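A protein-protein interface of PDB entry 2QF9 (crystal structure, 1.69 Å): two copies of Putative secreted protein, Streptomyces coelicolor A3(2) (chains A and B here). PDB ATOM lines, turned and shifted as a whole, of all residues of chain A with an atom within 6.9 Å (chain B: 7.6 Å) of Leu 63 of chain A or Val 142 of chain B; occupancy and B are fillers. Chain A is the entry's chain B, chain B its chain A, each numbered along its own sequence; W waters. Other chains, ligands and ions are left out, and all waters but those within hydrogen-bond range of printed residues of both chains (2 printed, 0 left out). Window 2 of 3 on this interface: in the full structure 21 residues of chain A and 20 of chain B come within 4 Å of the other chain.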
ATOM      1  N   ILE A  58       8.751 -11.992 -11.869  1.00  0.00           N
ATOM      2  CA  ILE A  58       8.380 -10.584 -11.703  1.00  0.00           C
ATOM      3  C   ILE A  58       9.632  -9.725 -11.474  1.00  0.00           C
ATOM      4  O   ILE A  58       9.757  -8.637 -12.065  1.00  0.00           O
ATOM      5  CB  ILE A  58       7.359 -10.413 -10.568  1.00  0.00           C
ATOM      6  CG1 ILE A  58       6.024 -11.034 -10.990  1.00  0.00           C
ATOM      7  CG2 ILE A  58       7.217  -8.934 -10.174  1.00  0.00           C
ATOM      8  CD1 ILE A  58       4.964 -10.946  -9.886  1.00  0.00           C
ATOM      9  N   GLY A  59      10.557 -10.217 -10.646  1.00  0.00           N
ATOM     10  CA  GLY A  59      11.831  -9.549 -10.408  1.00  0.00           C
ATOM     11  C   GLY A  59      12.608  -9.330 -11.702  1.00  0.00           C
ATOM     12  O   GLY A  59      13.226  -8.264 -11.884  1.00  0.00           O
ATOM     13  N   TRP A  60      12.607 -10.338 -12.582  1.00  0.00           N
ATOM     14  CA  TRP A  60      13.264 -10.189 -13.902  1.00  0.00           C
ATOM     15  C   TRP A  60      12.639  -9.070 -14.729  1.00  0.00           C
ATOM     16  O   TRP A  60      13.350  -8.204 -15.244  1.00  0.00           O
ATOM     17  CB  TRP A  60      13.290 -11.510 -14.681  1.00  0.00           C
ATOM     18  CG  TRP A  60      14.125 -12.593 -13.981  1.00  0.00           C
ATOM     19  CD1 TRP A  60      15.156 -12.406 -13.087  1.00  0.00           C
ATOM     20  CD2 TRP A  60      13.998 -14.005 -14.156  1.00  0.00           C
ATOM     21  NE1 TRP A  60      15.642 -13.626 -12.673  1.00  0.00           N
ATOM     22  CE2 TRP A  60      14.960 -14.622 -13.317  1.00  0.00           C
ATOM     23  CE3 TRP A  60      13.146 -14.816 -14.920  1.00  0.00           C
ATOM     24  CZ2 TRP A  60      15.100 -16.016 -13.231  1.00  0.00           C
ATOM     25  CZ3 TRP A  60      13.289 -16.208 -14.844  1.00  0.00           C
ATOM     26  CH2 TRP A  60      14.266 -16.791 -13.998  1.00  0.00           C
ATOM     27  N   LEU A  61      11.310  -9.078 -14.838  1.00  0.00           N
ATOM     28  CA  LEU A  61      10.584  -8.033 -15.559  1.00  0.00           C
ATOM     29  C   LEU A  61      10.933  -6.647 -14.990  1.00  0.00           C
ATOM     30  O   LEU A  61      11.234  -5.694 -15.730  1.00  0.00           O
ATOM     31  CB  LEU A  61       9.064  -8.297 -15.520  1.00  0.00           C
ATOM     32  CG  LEU A  61       8.544  -9.498 -16.350  1.00  0.00           C
ATOM     33  CD1 LEU A  61       7.066  -9.858 -16.017  1.00  0.00           C
ATOM     34  CD2 LEU A  61       8.737  -9.266 -17.855  1.00  0.00           C
ATOM     35  N   ASP A  62      10.932  -6.555 -13.668  1.00  0.00           N
ATOM     36  CA  ASP A  62      11.246  -5.282 -13.006  1.00  0.00           C
ATOM     37  C   ASP A  62      12.674  -4.835 -13.309  1.00  0.00           C
ATOM     38  O   ASP A  62      12.895  -3.673 -13.649  1.00  0.00           O
ATOM     39  CB  ASP A  62      11.001  -5.389 -11.497  1.00  0.00           C
ATOM     40  CG  ASP A  62       9.519  -5.347 -11.143  1.00  0.00           C
ATOM     41  OD1 ASP A  62       8.685  -4.991 -12.019  1.00  0.00           O
ATOM     42  OD2 ASP A  62       9.174  -5.634  -9.975  1.00  0.00           O
ATOM     43  N   LEU A  63      13.640  -5.746 -13.190  1.00  0.00           N
ATOM     44  CA  LEU A  63      15.032  -5.401 -13.491  1.00  0.00           C
ATOM     45  C   LEU A  63      15.209  -4.995 -14.961  1.00  0.00           C
ATOM     46  O   LEU A  63      15.958  -4.044 -15.284  1.00  0.00           O
ATOM     47  CB  LEU A  63      15.976  -6.535 -13.100  1.00  0.00           C
ATOM     48  CG  LEU A  63      17.453  -6.340 -13.459  1.00  0.00           C
ATOM     49  CD1 LEU A  63      18.103  -5.269 -12.617  1.00  0.00           C
ATOM     50  CD2 LEU A  63      18.185  -7.648 -13.327  1.00  0.00           C
ATOM     51  N   TRP A  64      14.504  -5.692 -15.845  1.00  0.00           N
ATOM     52  CA  TRP A  64      14.526  -5.400 -17.278  1.00  0.00           C
ATOM     53  C   TRP A  64      13.691  -4.176 -17.671  1.00  0.00           C
ATOM     54  O   TRP A  64      13.679  -3.794 -18.858  1.00  0.00           O
ATOM     55  CB  TRP A  64      14.076  -6.631 -18.081  1.00  0.00           C
ATOM     56  CG  TRP A  64      14.962  -7.829 -17.918  1.00  0.00           C
ATOM     57  CD1 TRP A  64      16.299  -7.841 -17.619  1.00  0.00           C
ATOM     58  CD2 TRP A  64      14.573  -9.192 -18.071  1.00  0.00           C
ATOM     59  NE1 TRP A  64      16.761  -9.136 -17.557  1.00  0.00           N
ATOM     60  CE2 TRP A  64      15.723  -9.986 -17.835  1.00  0.00           C
ATOM     61  CE3 TRP A  64      13.357  -9.825 -18.362  1.00  0.00           C
ATOM     62  CZ2 TRP A  64      15.693 -11.384 -17.895  1.00  0.00           C
ATOM     63  CZ3 TRP A  64      13.330 -11.234 -18.446  1.00  0.00           C
ATOM     64  CH2 TRP A  64      14.495 -11.989 -18.206  1.00  0.00           C
ATOM     65  N   ALA A  65      13.011  -3.567 -16.693  1.00  0.00           N
ATOM     66  CA  ALA A  65      12.136  -2.394 -16.912  1.00  0.00           C
ATOM     67  C   ALA A  65      11.021  -2.678 -17.930  1.00  0.00           C
ATOM     68  O   ALA A  65      10.673  -1.825 -18.765  1.00  0.00           O
ATOM     69  CB  ALA A  65      12.971  -1.150 -17.310  1.00  0.00           C
ATOM     70  N   LEU A  66      10.466  -3.884 -17.864  1.00  0.00           N
ATOM     71  CA  LEU A  66       9.363  -4.268 -18.740  1.00  0.00           C
ATOM     72  C   LEU A  66       8.069  -4.327 -17.946  1.00  0.00           C
ATOM     73  O   LEU A  66       8.073  -4.736 -16.776  1.00  0.00           O
ATOM     74  CB  LEU A  66       9.630  -5.620 -19.418  1.00  0.00           C
ATOM     75  CG  LEU A  66      10.888  -5.799 -20.270  1.00  0.00           C
ATOM     76  CD1 LEU A  66      11.024  -7.254 -20.716  1.00  0.00           C
ATOM     77  CD2 LEU A  66      10.879  -4.886 -21.490  1.00  0.00           C
ATOM     78  N   ASP B   9      24.473  -5.192  -2.715  1.00  0.00           N
ATOM     79  CA  ASP B   9      23.353  -5.733  -3.482  1.00  0.00           C
ATOM     80  C   ASP B   9      23.223  -7.237  -3.251  1.00  0.00           C
ATOM     81  O   ASP B   9      22.124  -7.728  -2.976  1.00  0.00           O
ATOM     82  CB  ASP B   9      23.527  -5.410  -4.958  1.00  0.00           C
ATOM     83  CG  ASP B   9      23.648  -3.909  -5.199  1.00  0.00           C
ATOM     84  OD1 ASP B   9      22.646  -3.208  -5.021  1.00  0.00           O
ATOM     85  OD2 ASP B   9      24.751  -3.446  -5.552  1.00  0.00           O
ATOM     86  N   MET B  56      11.866 -12.385  -5.898  1.00  0.00           N
ATOM     87  CA  MET B  56      12.545 -11.332  -6.678  1.00  0.00           C
ATOM     88  C   MET B  56      14.051 -11.332  -6.396  1.00  0.00           C
ATOM     89  O   MET B  56      14.873 -11.388  -7.318  1.00  0.00           O
ATOM     90  CB  MET B  56      11.949  -9.939  -6.391  1.00  0.00           C
ATOM     91  CG  MET B  56      10.526  -9.748  -6.896  1.00  0.00           C
ATOM     92  SD  MET B  56       9.864  -8.065  -6.148  1.00  0.00           S
ATOM     93  CE  MET B  56       8.200  -7.807  -7.104  1.00  0.00           C
ATOM     94  N   GLY B  59      15.773 -14.452  -7.533  1.00  0.00           N
ATOM     95  CA  GLY B  59      15.832 -14.352  -8.990  1.00  0.00           C
ATOM     96  C   GLY B  59      16.969 -13.450  -9.462  1.00  0.00           C
ATOM     97  O   GLY B  59      17.636 -13.737 -10.473  1.00  0.00           O
ATOM     98  N   TRP B  60      17.219 -12.376  -8.712  1.00  0.00           N
ATOM     99  CA  TRP B  60      18.347 -11.484  -9.041  1.00  0.00           C
ATOM    100  C   TRP B  60      19.668 -12.209  -8.848  1.00  0.00           C
ATOM    101  O   TRP B  60      20.539 -12.189  -9.726  1.00  0.00           O
ATOM    102  CB  TRP B  60      18.288 -10.159  -8.260  1.00  0.00           C
ATOM    103  CG  TRP B  60      17.071  -9.316  -8.592  1.00  0.00           C
ATOM    104  CD1 TRP B  60      16.341  -9.337  -9.758  1.00  0.00           C
ATOM    105  CD2 TRP B  60      16.446  -8.342  -7.750  1.00  0.00           C
ATOM    106  NE1 TRP B  60      15.298  -8.425  -9.691  1.00  0.00           N
ATOM    107  CE2 TRP B  60      15.341  -7.807  -8.469  1.00  0.00           C
ATOM    108  CE3 TRP B  60      16.717  -7.861  -6.459  1.00  0.00           C
ATOM    109  CZ2 TRP B  60      14.503  -6.815  -7.936  1.00  0.00           C
ATOM    110  CZ3 TRP B  60      15.869  -6.869  -5.923  1.00  0.00           C
ATOM    111  CH2 TRP B  60      14.779  -6.362  -6.666  1.00  0.00           C
ATOM    112  N   LEU B  63      20.084 -14.626 -11.730  1.00  0.00           N
ATOM    113  CA  LEU B  63      20.397 -13.906 -12.966  1.00  0.00           C
ATOM    114  C   LEU B  63      21.857 -13.393 -12.954  1.00  0.00           C
ATOM    115  O   LEU B  63      22.557 -13.411 -13.992  1.00  0.00           O
ATOM    116  CB  LEU B  63      19.431 -12.737 -13.141  1.00  0.00           C
ATOM    117  CG  LEU B  63      19.452 -11.930 -14.445  1.00  0.00           C
ATOM    118  CD1 LEU B  63      18.935 -12.740 -15.609  1.00  0.00           C
ATOM    119  CD2 LEU B  63      18.599 -10.691 -14.296  1.00  0.00           C
ATOM    120  N   TRP B  64      22.307 -12.974 -11.772  1.00  0.00           N
ATOM    121  CA  TRP B  64      23.667 -12.480 -11.577  1.00  0.00           C
ATOM    122  C   TRP B  64      24.717 -13.590 -11.405  1.00  0.00           C
ATOM    123  O   TRP B  64      25.908 -13.289 -11.251  1.00  0.00           O
ATOM    124  CB  TRP B  64      23.719 -11.540 -10.374  1.00  0.00           C
ATOM    125  CG  TRP B  64      22.878 -10.295 -10.511  1.00  0.00           C
ATOM    126  CD1 TRP B  64      22.541  -9.645 -11.673  1.00  0.00           C
ATOM    127  CD2 TRP B  64      22.326  -9.514  -9.446  1.00  0.00           C
ATOM    128  NE1 TRP B  64      21.785  -8.539 -11.397  1.00  0.00           N
ATOM    129  CE2 TRP B  64      21.647  -8.422 -10.037  1.00  0.00           C
ATOM    130  CE3 TRP B  64      22.323  -9.640  -8.048  1.00  0.00           C
ATOM    131  CZ2 TRP B  64      20.963  -7.454  -9.273  1.00  0.00           C
ATOM    132  CZ3 TRP B  64      21.644  -8.672  -7.283  1.00  0.00           C
ATOM    133  CH2 TRP B  64      20.988  -7.590  -7.903  1.00  0.00           C
ATOM    134  N   CYS B 134      20.382  -1.172   2.906  1.00  0.00           N
ATOM    135  CA  CYS B 134      20.389  -1.267   1.445  1.00  0.00           C
ATOM    136  C   CYS B 134      20.078   0.091   0.782  1.00  0.00           C
ATOM    137  O   CYS B 134      20.692   0.438  -0.224  1.00  0.00           O
ATOM    138  CB  CYS B 134      19.436  -2.369   0.967  1.00  0.00           C
ATOM    139  SG  CYS B 134      19.307  -2.594  -0.843  1.00  0.00           S
ATOM    140  N   THR B 139      23.481  -0.519  -4.903  1.00  0.00           N
ATOM    141  CA  THR B 139      23.747   0.217  -6.145  1.00  0.00           C
ATOM    142  C   THR B 139      22.752  -0.107  -7.277  1.00  0.00           C
ATOM    143  O   THR B 139      22.614   0.663  -8.235  1.00  0.00           O
ATOM    144  CB  THR B 139      25.209  -0.014  -6.640  1.00  0.00           C
ATOM    145  OG1 THR B 139      25.352  -1.353  -7.130  1.00  0.00           O
ATOM    146  CG2 THR B 139      26.219   0.211  -5.525  1.00  0.00           C
ATOM    147  N   VAL B 140      22.070  -1.248  -7.176  1.00  0.00           N
ATOM    148  CA  VAL B 140      21.096  -1.659  -8.180  1.00  0.00           C
ATOM    149  C   VAL B 140      19.747  -0.971  -7.930  1.00  0.00           C
ATOM    150  O   VAL B 140      19.148  -1.112  -6.853  1.00  0.00           O
ATOM    151  CB  VAL B 140      20.921  -3.211  -8.214  1.00  0.00           C
ATOM    152  CG1 VAL B 140      19.803  -3.598  -9.155  1.00  0.00           C
ATOM    153  CG2 VAL B 140      22.224  -3.902  -8.610  1.00  0.00           C
ATOM    154  N   GLY B 141      19.291  -0.220  -8.927  1.00  0.00           N
ATOM    155  CA  GLY B 141      18.136   0.658  -8.776  1.00  0.00           C
ATOM    156  C   GLY B 141      16.889  -0.058  -8.288  1.00  0.00           C
ATOM    157  O   GLY B 141      16.249   0.390  -7.336  1.00  0.00           O
ATOM    158  N   VAL B 142      16.545  -1.183  -8.930  1.00  0.00           N
ATOM    159  CA  VAL B 142      15.324  -1.900  -8.572  1.00  0.00           C
ATOM    160  C   VAL B 142      15.398  -2.445  -7.130  1.00  0.00           C
ATOM    161  O   VAL B 142      14.388  -2.492  -6.428  1.00  0.00           O
ATOM    162  CB  VAL B 142      14.982  -3.011  -9.611  1.00  0.00           C
ATOM    163  CG1 VAL B 142      16.084  -4.069  -9.694  1.00  0.00           C
ATOM    164  CG2 VAL B 142      13.641  -3.625  -9.332  1.00  0.00           C
ATOM    165  N   GLU B 143      16.598  -2.835  -6.716  1.00  0.00           N
ATOM    166  CA  GLU B 143      16.847  -3.343  -5.357  1.00  0.00           C
ATOM    167  C   GLU B 143      16.769  -2.240  -4.298  1.00  0.00           C
ATOM    168  O   GLU B 143      16.172  -2.445  -3.232  1.00  0.00           O
ATOM    169  CB  GLU B 143      18.187  -4.064  -5.283  1.00  0.00           C
ATOM    170  CG  GLU B 143      18.344  -4.867  -4.002  1.00  0.00           C
ATOM    171  CD  GLU B 143      19.580  -5.745  -3.983  1.00  0.00           C
ATOM    172  OE1 GLU B 143      20.289  -5.819  -5.009  1.00  0.00           O
ATOM    173  OE2 GLU B 143      19.829  -6.371  -2.934  1.00  0.00           O
ATOM    174  N   LYS B 144      17.380  -1.086  -4.589  1.00  0.00           N
ATOM    175  CA  LYS B 144      17.262   0.107  -3.733  1.00  0.00           C
ATOM    176  C   LYS B 144      15.792   0.504  -3.532  1.00  0.00           C
ATOM    177  O   LYS B 144      15.355   0.767  -2.404  1.00  0.00           O
ATOM    178  CB  LYS B 144      18.045   1.283  -4.331  1.00  0.00           C
ATOM    179  CG  LYS B 144      19.551   1.149  -4.196  1.00  0.00           C
ATOM    180  CD  LYS B 144      20.274   2.321  -4.861  1.00  0.00           C
ATOM    181  CE  LYS B 144      20.313   3.571  -3.979  1.00  0.00           C
ATOM    182  NZ  LYS B 144      20.711   4.790  -4.785  1.00  0.00           N
ATOM    183  N   ARG B 145      15.030   0.536  -4.625  1.00  0.00           N
ATOM    184  CA  ARG B 145      13.633   0.926  -4.569  1.00  0.00           C
ATOM    185  C   ARG B 145      12.813  -0.086  -3.793  1.00  0.00           C
ATOM    186  O   ARG B 145      11.902   0.294  -3.047  1.00  0.00           O
ATOM    187  CB  ARG B 145      13.061   1.128  -5.966  1.00  0.00           C
ATOM    188  CG  ARG B 145      13.691   2.325  -6.677  1.00  0.00           C
ATOM    189  CD  ARG B 145      12.898   2.772  -7.892  1.00  0.00           C
ATOM    190  NE  ARG B 145      12.715   1.697  -8.862  1.00  0.00           N
ATOM    191  CZ  ARG B 145      13.548   1.424  -9.866  1.00  0.00           C
ATOM    192  NH1 ARG B 145      14.649   2.149 -10.057  1.00  0.00           N
ATOM    193  NH2 ARG B 145      13.269   0.421 -10.689  1.00  0.00           N
ATOM    194  N   LEU B 146      13.146  -1.368  -3.965  1.00  0.00           N
ATOM    195  CA  LEU B 146      12.472  -2.422  -3.216  1.00  0.00           C
ATOM    196  C   LEU B 146      12.689  -2.230  -1.725  1.00  0.00           C
ATOM    197  O   LEU B 146      11.727  -2.289  -0.939  1.00  0.00           O
ATOM    198  CB  LEU B 146      12.932  -3.824  -3.649  1.00  0.00           C
ATOM    199  CG  LEU B 146      11.988  -4.968  -3.174  1.00  0.00           C
ATOM    200  CD1 LEU B 146      10.641  -4.954  -3.896  1.00  0.00           C
ATOM    201  CD2 LEU B 146      12.657  -6.313  -3.400  1.00  0.00           C
ATOM    202  N   ALA B 147      13.944  -1.981  -1.352  1.00  0.00           N
ATOM    203  CA  ALA B 147      14.327  -1.740   0.043  1.00  0.00           C
ATOM    204  C   ALA B 147      13.581  -0.519   0.625  1.00  0.00           C
ATOM    205  O   ALA B 147      13.039  -0.577   1.729  1.00  0.00           O
ATOM    206  CB  ALA B 147      15.848  -1.575   0.146  1.00  0.00           C
ATOM    207  N   ARG B 148      13.538   0.572  -0.140  1.00  0.00           N
ATOM    208  CA  ARG B 148      12.837   1.797   0.277  1.00  0.00           C
ATOM    209  C   ARG B 148      11.338   1.530   0.523  1.00  0.00           C
ATOM    210  O   ARG B 148      10.731   2.101   1.440  1.00  0.00           O
ATOM    211  CB  ARG B 148      13.055   2.888  -0.781  1.00  0.00           C
ATOM    212  CG  ARG B 148      12.928   4.335  -0.295  1.00  0.00           C
ATOM    213  CD  ARG B 148      14.043   5.217  -0.894  1.00  0.00           C
ATOM    214  NE  ARG B 148      14.413   4.831  -2.260  1.00  0.00           N
ATOM    215  CZ  ARG B 148      15.609   5.032  -2.808  1.00  0.00           C
ATOM    216  NH1 ARG B 148      16.577   5.614  -2.112  1.00  0.00           N
ATOM    217  NH2 ARG B 148      15.838   4.643  -4.056  1.00  0.00           N
HETATM  218  O   HOH W   1      14.278 -11.741 -10.085  1.00  0.00           O
HETATM  219  O   HOH W   2      11.162  -5.470  -8.064  1.00  0.00           O
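The indole nitrogen (NE1) of Trp 60 of chain A sits at hydrogen-bond distance from the backbone carbonyl oxygen (O) of Gly 59 of chain B (3.0 Å). The indole nitrogen of Trp 60 of chain B sits at hydrogen-bond distance from the backbone carbonyl oxygen of Gly 59 of chain A, at 3.0 Å.
Among the printed residues, pairs that only touch across the chains: Ile 58 of chain A with Met 56 of chain B, Gly 59 of chain A with Met 56 of chain B, Trp 60 of chain A with Leu 63 of chain B, Asp 62 of chain A with Met 56 of chain B, Asp 62 of chain A with Val 142 of chain B, Leu 63 of chain A with Trp 60 of chain B, Leu 63 of chain A with Leu 63 of chain B and Leu 63 of chain A with Val 142 of chain B.
Of the printed residues of chain B, Leu 63 of chain A touches Trp 60 (3.96 Å), Leu 63 (3.2 Å) and Val 142 (3.7 Å). Val 142 of chain B touches two residues of chain A. Of the printed residues of chain A, Gly 59 of chain B touches Trp 60. Of the printed residues of chain B, Trp 60 of chain A touches Gly 59 (3.0 Å) and Leu 63 (3.9 Å). Of the printed residues of chain B, Ile 58 of chain A touches Met 56 (3.4 Å). Trp 64 of chain B touches none of the printed residues of chain A.
Printed residues of chain A that touch a printed residue of chain B: Ile 58, Gly 59, Trp 60, Asp 62 and Leu 63. Hydrophobic or aromatic side chains of chain A that line the printed part of chain B: Ile 58, Trp 60 and Leu 63. Printed residues of chain B that touch a printed residue of chain A: Met 56, Gly 59, Trp 60, Leu 63 and Val 142. Hydrophobic or aromatic side chains of chain B within 4 Å of the printed part of chain A: Met 56, Trp 60, Leu 63 and Val 142. Among the printed residues, no Asp or Glu carboxylate lies within 4 Å of a Lys or Arg side-chain nitrogen of the other chain.
Gly 59 of chain A touches Trp 60 of chain B, and with the chains exchanged Trp 60 of chain A touches Gly 59 of chain B. Trp 60 of chain A touches Leu 63 of chain B, and with the chains exchanged Leu 63 of chain A touches Trp 60 of chain B. Leu 63 of chain A touches its own counterpart, Leu 63 of chain B. Of the 10 pairs that touch across the chains among the printed residues, 5 have their exchanged pair printed and touching as well.
Water W2 bridges the side-chain carboxylate of Asp 62 of chain A (2.8 Å) and the side-chain sulfur of Met 56 of chain B (3.5 Å). Water W1 lies within hydrogen-bond range of O of Met 56 of chain B (2.9 Å), N of Trp 60 of chain B (3.3 Å) and N of Trp 60 of chain A (3.3 Å).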
